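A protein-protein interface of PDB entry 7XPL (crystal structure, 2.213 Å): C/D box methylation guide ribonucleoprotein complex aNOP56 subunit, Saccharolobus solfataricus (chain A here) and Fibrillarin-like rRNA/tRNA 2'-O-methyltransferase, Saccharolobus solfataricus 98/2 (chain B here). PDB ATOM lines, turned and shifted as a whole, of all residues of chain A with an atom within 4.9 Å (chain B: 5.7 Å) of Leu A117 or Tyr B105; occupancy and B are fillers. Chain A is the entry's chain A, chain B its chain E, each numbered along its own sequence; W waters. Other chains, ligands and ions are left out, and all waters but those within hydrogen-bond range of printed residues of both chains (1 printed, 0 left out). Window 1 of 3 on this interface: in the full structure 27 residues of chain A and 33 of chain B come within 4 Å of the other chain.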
ATOM      1  N   VAL A  10      40.474  26.939 -20.935  1.00  0.00           N
ATOM      2  CA  VAL A  10      40.840  28.183 -21.602  1.00  0.00           C
ATOM      3  C   VAL A  10      41.558  29.127 -20.628  1.00  0.00           C
ATOM      4  O   VAL A  10      42.589  29.719 -20.966  1.00  0.00           O
ATOM      5  CB  VAL A  10      39.587  28.859 -22.206  1.00  0.00           C
ATOM      6  CG1 VAL A  10      39.849  30.346 -22.517  1.00  0.00           C
ATOM      7  CG2 VAL A  10      39.107  28.115 -23.465  1.00  0.00           C
ATOM      8  N   TYR A 113      35.428  38.225 -20.200  1.00  0.00           N
ATOM      9  CA  TYR A 113      35.661  36.788 -20.290  1.00  0.00           C
ATOM     10  C   TYR A 113      34.907  36.174 -21.474  1.00  0.00           C
ATOM     11  O   TYR A 113      35.490  35.443 -22.285  1.00  0.00           O
ATOM     12  CB  TYR A 113      35.263  36.114 -18.976  1.00  0.00           C
ATOM     13  CG  TYR A 113      35.185  34.625 -19.110  1.00  0.00           C
ATOM     14  CD1 TYR A 113      36.337  33.861 -19.211  1.00  0.00           C
ATOM     15  CD2 TYR A 113      33.959  33.974 -19.178  1.00  0.00           C
ATOM     16  CE1 TYR A 113      36.263  32.488 -19.361  1.00  0.00           C
ATOM     17  CE2 TYR A 113      33.880  32.598 -19.335  1.00  0.00           C
ATOM     18  CZ  TYR A 113      35.037  31.864 -19.414  1.00  0.00           C
ATOM     19  OH  TYR A 113      34.977  30.503 -19.562  1.00  0.00           O
ATOM     20  N   TYR A 114      33.616  36.484 -21.603  1.00  0.00           N
ATOM     21  CA  TYR A 114      32.809  35.923 -22.682  1.00  0.00           C
ATOM     22  C   TYR A 114      33.159  36.501 -24.049  1.00  0.00           C
ATOM     23  O   TYR A 114      33.102  35.773 -25.046  1.00  0.00           O
ATOM     24  CB  TYR A 114      31.330  36.128 -22.388  1.00  0.00           C
ATOM     25  CG  TYR A 114      30.840  35.198 -21.306  1.00  0.00           C
ATOM     26  CD1 TYR A 114      30.836  33.816 -21.497  1.00  0.00           C
ATOM     27  CD2 TYR A 114      30.380  35.690 -20.094  1.00  0.00           C
ATOM     28  CE1 TYR A 114      30.373  32.946 -20.507  1.00  0.00           C
ATOM     29  CE2 TYR A 114      29.921  34.834 -19.098  1.00  0.00           C
ATOM     30  CZ  TYR A 114      29.916  33.469 -19.302  1.00  0.00           C
ATOM     31  OH  TYR A 114      29.446  32.646 -18.291  1.00  0.00           O
ATOM     32  N   ASN A 115      33.512  37.785 -24.138  1.00  0.00           N
ATOM     33  CA  ASN A 115      34.046  38.280 -25.402  1.00  0.00           C
ATOM     34  C   ASN A 115      35.190  37.388 -25.875  1.00  0.00           C
ATOM     35  O   ASN A 115      35.206  36.926 -27.021  1.00  0.00           O
ATOM     36  CB  ASN A 115      34.526  39.729 -25.275  1.00  0.00           C
ATOM     37  CG  ASN A 115      33.378  40.737 -25.150  1.00  0.00           C
ATOM     38  OD1 ASN A 115      32.300  40.564 -25.734  1.00  0.00           O
ATOM     39  ND2 ASN A 115      33.617  41.808 -24.389  1.00  0.00           N
ATOM     40  N   PHE A 116      36.155  37.117 -24.990  1.00  0.00           N
ATOM     41  CA  PHE A 116      37.316  36.321 -25.391  1.00  0.00           C
ATOM     42  C   PHE A 116      36.935  34.869 -25.645  1.00  0.00           C
ATOM     43  O   PHE A 116      37.429  34.250 -26.590  1.00  0.00           O
ATOM     44  CB  PHE A 116      38.407  36.405 -24.330  1.00  0.00           C
ATOM     45  CG  PHE A 116      39.670  35.713 -24.723  1.00  0.00           C
ATOM     46  CD1 PHE A 116      39.855  34.352 -24.460  1.00  0.00           C
ATOM     47  CD2 PHE A 116      40.672  36.410 -25.379  1.00  0.00           C
ATOM     48  CE1 PHE A 116      41.007  33.718 -24.836  1.00  0.00           C
ATOM     49  CE2 PHE A 116      41.849  35.770 -25.746  1.00  0.00           C
ATOM     50  CZ  PHE A 116      42.014  34.421 -25.473  1.00  0.00           C
ATOM     51  N   LEU A 117      36.058  34.311 -24.817  1.00  0.00           N
ATOM     52  CA  LEU A 117      35.670  32.920 -25.009  1.00  0.00           C
ATOM     53  C   LEU A 117      35.044  32.723 -26.373  1.00  0.00           C
ATOM     54  O   LEU A 117      35.345  31.744 -27.068  1.00  0.00           O
ATOM     55  CB  LEU A 117      34.702  32.492 -23.914  1.00  0.00           C
ATOM     56  CG  LEU A 117      34.463  30.988 -23.911  1.00  0.00           C
ATOM     57  CD1 LEU A 117      35.762  30.240 -23.540  1.00  0.00           C
ATOM     58  CD2 LEU A 117      33.342  30.632 -22.978  1.00  0.00           C
ATOM     59  N   HIS A 118      34.192  33.674 -26.787  1.00  0.00           N
ATOM     60  CA  HIS A 118      33.539  33.593 -28.089  1.00  0.00           C
ATOM     61  C   HIS A 118      34.563  33.605 -29.213  1.00  0.00           C
ATOM     62  O   HIS A 118      34.514  32.767 -30.120  1.00  0.00           O
ATOM     63  CB  HIS A 118      32.537  34.743 -28.267  1.00  0.00           C
ATOM     64  CG  HIS A 118      31.625  34.547 -29.435  1.00  0.00           C
ATOM     65  ND1 HIS A 118      31.764  35.240 -30.620  1.00  0.00           N
ATOM     66  CD2 HIS A 118      30.602  33.675 -29.626  1.00  0.00           C
ATOM     67  CE1 HIS A 118      30.854  34.822 -31.480  1.00  0.00           C
ATOM     68  NE2 HIS A 118      30.142  33.867 -30.906  1.00  0.00           N
ATOM     69  N   GLU A 119      35.513  34.538 -29.171  1.00  0.00           N
ATOM     70  CA  GLU A 119      36.530  34.545 -30.216  1.00  0.00           C
ATOM     71  C   GLU A 119      37.344  33.255 -30.191  1.00  0.00           C
ATOM     72  O   GLU A 119      37.682  32.707 -31.251  1.00  0.00           O
ATOM     73  CB  GLU A 119      37.419  35.782 -30.073  1.00  0.00           C
ATOM     74  CG  GLU A 119      36.630  37.110 -30.212  1.00  0.00           C
ATOM     75  CD  GLU A 119      35.900  37.286 -31.586  1.00  0.00           C
ATOM     76  OE1 GLU A 119      36.527  37.034 -32.641  1.00  0.00           O
ATOM     77  OE2 GLU A 119      34.699  37.678 -31.599  1.00  0.00           O
ATOM     78  N   LEU A 120      37.621  32.725 -28.988  1.00  0.00           N
ATOM     79  CA  LEU A 120      38.327  31.457 -28.874  1.00  0.00           C
ATOM     80  C   LEU A 120      37.560  30.337 -29.563  1.00  0.00           C
ATOM     81  O   LEU A 120      38.128  29.583 -30.363  1.00  0.00           O
ATOM     82  CB  LEU A 120      38.576  31.126 -27.396  1.00  0.00           C
ATOM     83  CG  LEU A 120      39.446  29.927 -26.971  1.00  0.00           C
ATOM     84  CD1 LEU A 120      38.671  28.616 -27.023  1.00  0.00           C
ATOM     85  CD2 LEU A 120      40.716  29.842 -27.821  1.00  0.00           C
ATOM     86  N   SER A 121      36.268  30.201 -29.259  1.00  0.00           N
ATOM     87  CA  SER A 121      35.507  29.103 -29.853  1.00  0.00           C
ATOM     88  C   SER A 121      35.502  29.196 -31.375  1.00  0.00           C
ATOM     89  O   SER A 121      35.607  28.170 -32.058  1.00  0.00           O
ATOM     90  CB  SER A 121      34.083  29.067 -29.295  1.00  0.00           C
ATOM     91  OG  SER A 121      33.354  30.241 -29.605  1.00  0.00           O
ATOM     92  N   LYS B  79      21.761  29.066 -19.460  1.00  0.00           N
ATOM     93  CA  LYS B  79      22.962  28.441 -20.003  1.00  0.00           C
ATOM     94  C   LYS B  79      22.619  27.047 -20.513  1.00  0.00           C
ATOM     95  O   LYS B  79      22.081  26.224 -19.769  1.00  0.00           O
ATOM     96  CB  LYS B  79      24.069  28.367 -18.946  1.00  0.00           C
ATOM     97  CG  LYS B  79      24.780  29.700 -18.766  1.00  0.00           C
ATOM     98  CD  LYS B  79      25.650  29.764 -17.526  1.00  0.00           C
ATOM     99  CE  LYS B  79      26.366  31.120 -17.501  1.00  0.00           C
ATOM    100  NZ  LYS B  79      27.471  31.191 -16.494  1.00  0.00           N
ATOM    101  N   VAL B  80      22.944  26.780 -21.779  1.00  0.00           N
ATOM    102  CA  VAL B  80      22.508  25.564 -22.457  1.00  0.00           C
ATOM    103  C   VAL B  80      23.692  24.919 -23.167  1.00  0.00           C
ATOM    104  O   VAL B  80      24.491  25.601 -23.822  1.00  0.00           O
ATOM    105  CB  VAL B  80      21.353  25.852 -23.452  1.00  0.00           C
ATOM    106  CG1 VAL B  80      21.699  26.983 -24.333  1.00  0.00           C
ATOM    107  CG2 VAL B  80      20.995  24.620 -24.284  1.00  0.00           C
ATOM    108  N   LEU B  81      23.815  23.602 -23.004  1.00  0.00           N
ATOM    109  CA  LEU B  81      24.700  22.776 -23.814  1.00  0.00           C
ATOM    110  C   LEU B  81      23.842  22.145 -24.894  1.00  0.00           C
ATOM    111  O   LEU B  81      22.886  21.420 -24.589  1.00  0.00           O
ATOM    112  CB  LEU B  81      25.390  21.694 -22.987  1.00  0.00           C
ATOM    113  CG  LEU B  81      26.345  20.762 -23.724  1.00  0.00           C
ATOM    114  CD1 LEU B  81      27.373  21.584 -24.475  1.00  0.00           C
ATOM    115  CD2 LEU B  81      27.022  19.825 -22.715  1.00  0.00           C
ATOM    116  N   TYR B  82      24.177  22.436 -26.146  1.00  0.00           N
ATOM    117  CA  TYR B  82      23.393  22.008 -27.291  1.00  0.00           C
ATOM    118  C   TYR B  82      24.229  20.974 -28.030  1.00  0.00           C
ATOM    119  O   TYR B  82      25.251  21.310 -28.642  1.00  0.00           O
ATOM    120  CB  TYR B  82      23.033  23.211 -28.170  1.00  0.00           C
ATOM    121  CG  TYR B  82      21.953  22.983 -29.206  1.00  0.00           C
ATOM    122  CD1 TYR B  82      22.009  21.909 -30.093  1.00  0.00           C
ATOM    123  CD2 TYR B  82      20.876  23.862 -29.315  1.00  0.00           C
ATOM    124  CE1 TYR B  82      21.011  21.708 -31.056  1.00  0.00           C
ATOM    125  CE2 TYR B  82      19.881  23.674 -30.273  1.00  0.00           C
ATOM    126  CZ  TYR B  82      19.957  22.602 -31.144  1.00  0.00           C
ATOM    127  OH  TYR B  82      18.967  22.413 -32.083  1.00  0.00           O
ATOM    128  N   LEU B  83      23.803  19.719 -27.959  1.00  0.00           N
ATOM    129  CA  LEU B  83      24.458  18.625 -28.660  1.00  0.00           C
ATOM    130  C   LEU B  83      23.696  18.384 -29.956  1.00  0.00           C
ATOM    131  O   LEU B  83      22.481  18.145 -29.924  1.00  0.00           O
ATOM    132  CB  LEU B  83      24.478  17.363 -27.799  1.00  0.00           C
ATOM    133  CG  LEU B  83      25.034  17.442 -26.367  1.00  0.00           C
ATOM    134  CD1 LEU B  83      25.071  16.031 -25.782  1.00  0.00           C
ATOM    135  CD2 LEU B  83      26.431  18.077 -26.300  1.00  0.00           C
ATOM    136  N   ILE B  91      19.288  26.318 -32.878  1.00  0.00           N
ATOM    137  CA  ILE B  91      20.111  27.031 -31.900  1.00  0.00           C
ATOM    138  C   ILE B  91      20.040  28.547 -32.113  1.00  0.00           C
ATOM    139  O   ILE B  91      20.203  29.313 -31.153  1.00  0.00           O
ATOM    140  CB  ILE B  91      21.574  26.508 -31.902  1.00  0.00           C
ATOM    141  CG1 ILE B  91      22.296  26.936 -30.614  1.00  0.00           C
ATOM    142  CG2 ILE B  91      22.362  26.982 -33.132  1.00  0.00           C
ATOM    143  CD1 ILE B  91      23.596  26.144 -30.300  1.00  0.00           C
ATOM    144  N   LYS B 103      23.940  31.779 -22.507  1.00  0.00           N
ATOM    145  CA  LYS B 103      25.017  31.176 -23.286  1.00  0.00           C
ATOM    146  C   LYS B 103      24.543  29.852 -23.849  1.00  0.00           C
ATOM    147  O   LYS B 103      23.931  29.048 -23.137  1.00  0.00           O
ATOM    148  CB  LYS B 103      26.276  30.932 -22.453  1.00  0.00           C
ATOM    149  CG  LYS B 103      26.683  32.106 -21.606  1.00  0.00           C
ATOM    150  CD  LYS B 103      27.224  33.246 -22.436  1.00  0.00           C
ATOM    151  CE  LYS B 103      27.200  34.539 -21.628  1.00  0.00           C
ATOM    152  NZ  LYS B 103      27.114  35.734 -22.505  1.00  0.00           N
ATOM    153  N   ALA B 104      24.846  29.634 -25.128  1.00  0.00           N
ATOM    154  CA  ALA B 104      24.496  28.414 -25.844  1.00  0.00           C
ATOM    155  C   ALA B 104      25.769  27.806 -26.428  1.00  0.00           C
ATOM    156  O   ALA B 104      26.356  28.364 -27.364  1.00  0.00           O
ATOM    157  CB  ALA B 104      23.484  28.712 -26.944  1.00  0.00           C
ATOM    158  N   TYR B 105      26.189  26.670 -25.888  1.00  0.00           N
ATOM    159  CA  TYR B 105      27.377  25.984 -26.364  1.00  0.00           C
ATOM    160  C   TYR B 105      26.922  24.940 -27.373  1.00  0.00           C
ATOM    161  O   TYR B 105      26.154  24.029 -27.033  1.00  0.00           O
ATOM    162  CB  TYR B 105      28.140  25.354 -25.192  1.00  0.00           C
ATOM    163  CG  TYR B 105      28.632  26.367 -24.170  1.00  0.00           C
ATOM    164  CD1 TYR B 105      27.860  26.700 -23.060  1.00  0.00           C
ATOM    165  CD2 TYR B 105      29.857  26.999 -24.327  1.00  0.00           C
ATOM    166  CE1 TYR B 105      28.304  27.623 -22.121  1.00  0.00           C
ATOM    167  CE2 TYR B 105      30.314  27.919 -23.405  1.00  0.00           C
ATOM    168  CZ  TYR B 105      29.540  28.226 -22.295  1.00  0.00           C
ATOM    169  OH  TYR B 105      30.001  29.151 -21.363  1.00  0.00           O
ATOM    170  N   GLY B 106      27.362  25.094 -28.614  1.00  0.00           N
ATOM    171  CA  GLY B 106      26.877  24.253 -29.689  1.00  0.00           C
ATOM    172  C   GLY B 106      27.894  23.223 -30.136  1.00  0.00           C
ATOM    173  O   GLY B 106      28.925  23.573 -30.712  1.00  0.00           O
ATOM    174  N   VAL B 107      27.602  21.948 -29.876  1.00  0.00           N
ATOM    175  CA  VAL B 107      28.476  20.830 -30.200  1.00  0.00           C
ATOM    176  C   VAL B 107      27.951  20.175 -31.473  1.00  0.00           C
ATOM    177  O   VAL B 107      26.768  19.837 -31.557  1.00  0.00           O
ATOM    178  CB  VAL B 107      28.532  19.827 -29.029  1.00  0.00           C
ATOM    179  CG1 VAL B 107      29.352  18.570 -29.403  1.00  0.00           C
ATOM    180  CG2 VAL B 107      29.156  20.485 -27.814  1.00  0.00           C
ATOM    181  N   ASN B 126      26.189  35.117 -28.350  1.00  0.00           N
ATOM    182  CA  ASN B 126      25.414  34.104 -27.644  1.00  0.00           C
ATOM    183  C   ASN B 126      25.924  32.676 -27.807  1.00  0.00           C
ATOM    184  O   ASN B 126      25.631  31.816 -26.969  1.00  0.00           O
ATOM    185  CB  ASN B 126      23.988  34.167 -28.210  1.00  0.00           C
ATOM    186  CG  ASN B 126      23.003  34.492 -27.177  1.00  0.00           C
ATOM    187  OD1 ASN B 126      23.375  34.779 -26.047  1.00  0.00           O
ATOM    188  ND2 ASN B 126      21.740  34.450 -27.518  1.00  0.00           N
ATOM    189  N   ILE B 127      26.560  32.371 -28.930  1.00  0.00           N
ATOM    190  CA  ILE B 127      26.686  31.000 -29.421  1.00  0.00           C
ATOM    191  C   ILE B 127      28.155  30.675 -29.580  1.00  0.00           C
ATOM    192  O   ILE B 127      28.871  31.362 -30.319  1.00  0.00           O
ATOM    193  CB  ILE B 127      25.968  30.804 -30.767  1.00  0.00           C
ATOM    194  CG1 ILE B 127      24.455  30.958 -30.601  1.00  0.00           C
ATOM    195  CG2 ILE B 127      26.342  29.451 -31.419  1.00  0.00           C
ATOM    196  CD1 ILE B 127      23.722  30.710 -31.899  1.00  0.00           C
ATOM    197  N   PHE B 128      28.575  29.595 -28.943  1.00  0.00           N
ATOM    198  CA  PHE B 128      29.961  29.143 -28.948  1.00  0.00           C
ATOM    199  C   PHE B 128      30.016  27.824 -29.708  1.00  0.00           C
ATOM    200  O   PHE B 128      29.654  26.769 -29.154  1.00  0.00           O
ATOM    201  CB  PHE B 128      30.461  28.992 -27.505  1.00  0.00           C
ATOM    202  CG  PHE B 128      30.303  30.262 -26.679  1.00  0.00           C
ATOM    203  CD1 PHE B 128      29.060  30.639 -26.189  1.00  0.00           C
ATOM    204  CD2 PHE B 128      31.390  31.096 -26.439  1.00  0.00           C
ATOM    205  CE1 PHE B 128      28.896  31.831 -25.462  1.00  0.00           C
ATOM    206  CE2 PHE B 128      31.242  32.290 -25.709  1.00  0.00           C
ATOM    207  CZ  PHE B 128      29.994  32.652 -25.215  1.00  0.00           C
ATOM    208  N   LEU B 130      31.309  24.431 -31.273  1.00  0.00           N
ATOM    209  CA  LEU B 130      32.339  23.455 -30.922  1.00  0.00           C
ATOM    210  C   LEU B 130      32.259  22.284 -31.891  1.00  0.00           C
ATOM    211  O   LEU B 130      31.340  21.459 -31.800  1.00  0.00           O
ATOM    212  CB  LEU B 130      32.168  22.995 -29.484  1.00  0.00           C
ATOM    213  CG  LEU B 130      32.340  24.138 -28.474  1.00  0.00           C
ATOM    214  CD1 LEU B 130      31.779  23.763 -27.113  1.00  0.00           C
ATOM    215  CD2 LEU B 130      33.808  24.560 -28.376  1.00  0.00           C
ATOM    216  N   VAL B 143      36.454  24.322 -22.679  1.00  0.00           N
ATOM    217  CA  VAL B 143      35.866  25.552 -23.183  1.00  0.00           C
ATOM    218  C   VAL B 143      34.575  25.884 -22.459  1.00  0.00           C
ATOM    219  O   VAL B 143      34.350  27.041 -22.077  1.00  0.00           O
ATOM    220  CB  VAL B 143      35.624  25.472 -24.704  1.00  0.00           C
ATOM    221  CG1 VAL B 143      34.777  26.639 -25.166  1.00  0.00           C
ATOM    222  CG2 VAL B 143      36.944  25.435 -25.449  1.00  0.00           C
ATOM    223  N   VAL B 144      33.744  24.876 -22.203  1.00  0.00           N
ATOM    224  CA  VAL B 144      32.395  25.135 -21.728  1.00  0.00           C
ATOM    225  C   VAL B 144      32.415  25.426 -20.234  1.00  0.00           C
ATOM    226  O   VAL B 144      33.468  25.700 -19.646  1.00  0.00           O
ATOM    227  CB  VAL B 144      31.451  23.965 -22.061  1.00  0.00           C
ATOM    228  CG1 VAL B 144      31.408  23.730 -23.582  1.00  0.00           C
ATOM    229  CG2 VAL B 144      31.924  22.743 -21.400  1.00  0.00           C
ATOM    230  N   GLU B 145      31.229  25.411 -19.634  1.00  0.00           N
ATOM    231  CA  GLU B 145      31.006  25.598 -18.215  1.00  0.00           C
ATOM    232  C   GLU B 145      29.807  24.721 -17.886  1.00  0.00           C
ATOM    233  O   GLU B 145      29.263  24.050 -18.767  1.00  0.00           O
ATOM    234  CB  GLU B 145      30.789  27.083 -17.898  1.00  0.00           C
ATOM    235  CG  GLU B 145      29.408  27.574 -18.278  1.00  0.00           C
ATOM    236  CD  GLU B 145      29.206  29.060 -18.023  1.00  0.00           C
ATOM    237  OE1 GLU B 145      29.122  29.845 -19.021  1.00  0.00           O
ATOM    238  OE2 GLU B 145      29.114  29.442 -16.828  1.00  0.00           O
ATOM    239  N   ASN B 146      29.391  24.691 -16.629  1.00  0.00           N
ATOM    240  CA  ASN B 146      28.171  23.930 -16.412  1.00  0.00           C
ATOM    241  C   ASN B 146      26.941  24.760 -16.786  1.00  0.00           C
ATOM    242  O   ASN B 146      26.992  25.988 -16.892  1.00  0.00           O
ATOM    243  CB  ASN B 146      28.102  23.428 -14.976  1.00  0.00           C
ATOM    244  CG  ASN B 146      28.887  22.139 -14.798  1.00  0.00           C
ATOM    245  OD1 ASN B 146      29.837  21.875 -15.538  1.00  0.00           O
ATOM    246  ND2 ASN B 146      28.457  21.306 -13.860  1.00  0.00           N
ATOM    247  N   VAL B 147      25.822  24.068 -17.010  1.00  0.00           N
ATOM    248  CA  VAL B 147      24.684  24.671 -17.694  1.00  0.00           C
ATOM    249  C   VAL B 147      23.386  24.277 -17.010  1.00  0.00           C
ATOM    250  O   VAL B 147      23.299  23.252 -16.326  1.00  0.00           O
ATOM    251  CB  VAL B 147      24.625  24.254 -19.185  1.00  0.00           C
ATOM    252  CG1 VAL B 147      25.802  24.848 -19.940  1.00  0.00           C
ATOM    253  CG2 VAL B 147      24.632  22.712 -19.276  1.00  0.00           C
HETATM  254  O   HOH W   1      32.745  28.579 -20.357  1.00  0.00           O
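Water W1 lies within hydrogen-bond range of O of Val B143, OH of Tyr B105, OH of Tyr A113 and O of Val B144.
OE2 of Glu B145 lies within salt-bridge range of NZ of Lys B79. The backbone NH of Val B80 sits at hydrogen-bond distance from the backbone carbonyl oxygen of Lys B103. O of Tyr B105 sits at hydrogen-bond distance from N of Tyr B82, at 2.7 Å. The backbone carbonyl oxygen (O) of Ala B104 is in hydrogen-bond range of the backbone NH (N) of Phe B128 (3.0 Å). The side-chain hydroxyl (OH) of Tyr B105 sits at hydrogen-bond distance from the side-chain carboxylate (OE1) of Glu B145 (2.6 Å). The backbone NH (N) of Gly B106 lies within hydrogen-bond range of the backbone carbonyl oxygen (O) of Phe B128 (2.9 Å).
Among the printed residues, pairs that only touch across the chains: His A118 with Phe B128, Ser A121 with Phe B128, Tyr A114 with Lys B103, Leu A117 with Val B143, Leu A117 with Phe B128, Tyr A114 with Tyr B105, Leu A120 with Val B143, Val A10 with Val B143, Tyr A114 with Phe B128 and Leu A117 with Tyr B105.
OH of Tyr A114 sits at hydrogen-bond distance from NZ of Lys B79. The side-chain hydroxyl of Tyr A114 lies within hydrogen-bond range of the side-chain carboxylate of Glu B145 (2.9 Å). A ring nitrogen (NE2) of His A118 lies within hydrogen-bond range of the backbone carbonyl oxygen of Ile B127 (2.9 Å).
Of the printed residues of chain B, Leu A117 touches Tyr B105 (3.995 Å), Phe B128 (3.8 Å) and Val B143 (3.8 Å). Of the printed residues of chain A, Tyr B105 touches Tyr A114 and Leu A117. Of the printed residues of chain A, Ile B127 touches His A118 (2.9 Å). Of the printed residues of chain A, Lys B79 touches Tyr A114. Printed residues of chain A within 4 Å of Phe B128: Tyr A114, Leu A117, His A118 and Ser A121. Ala B104 touches none of the printed residues of chain A. The nearest printed residue of chain B that does not touch Leu A117 is Val B144 (5.7 Å). The nearest printed residue of chain A that does not touch Tyr B105 is Tyr A113 (5.5 Å).
Of the 10 printed residues of chain A, 6 touch a printed residue of chain B. Printed residues of chain A that touch a printed residue of chain B: Val A10, Tyr A114, Leu A117, His A118, Leu A120 and Ser A121. Hydrophobic or aromatic side chains of chain A within 4 Å of the printed part of chain B: Val A10, Tyr A114, Leu A117, His A118 and Leu A120. Among the printed residues, 13 pairs touch across the chains.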
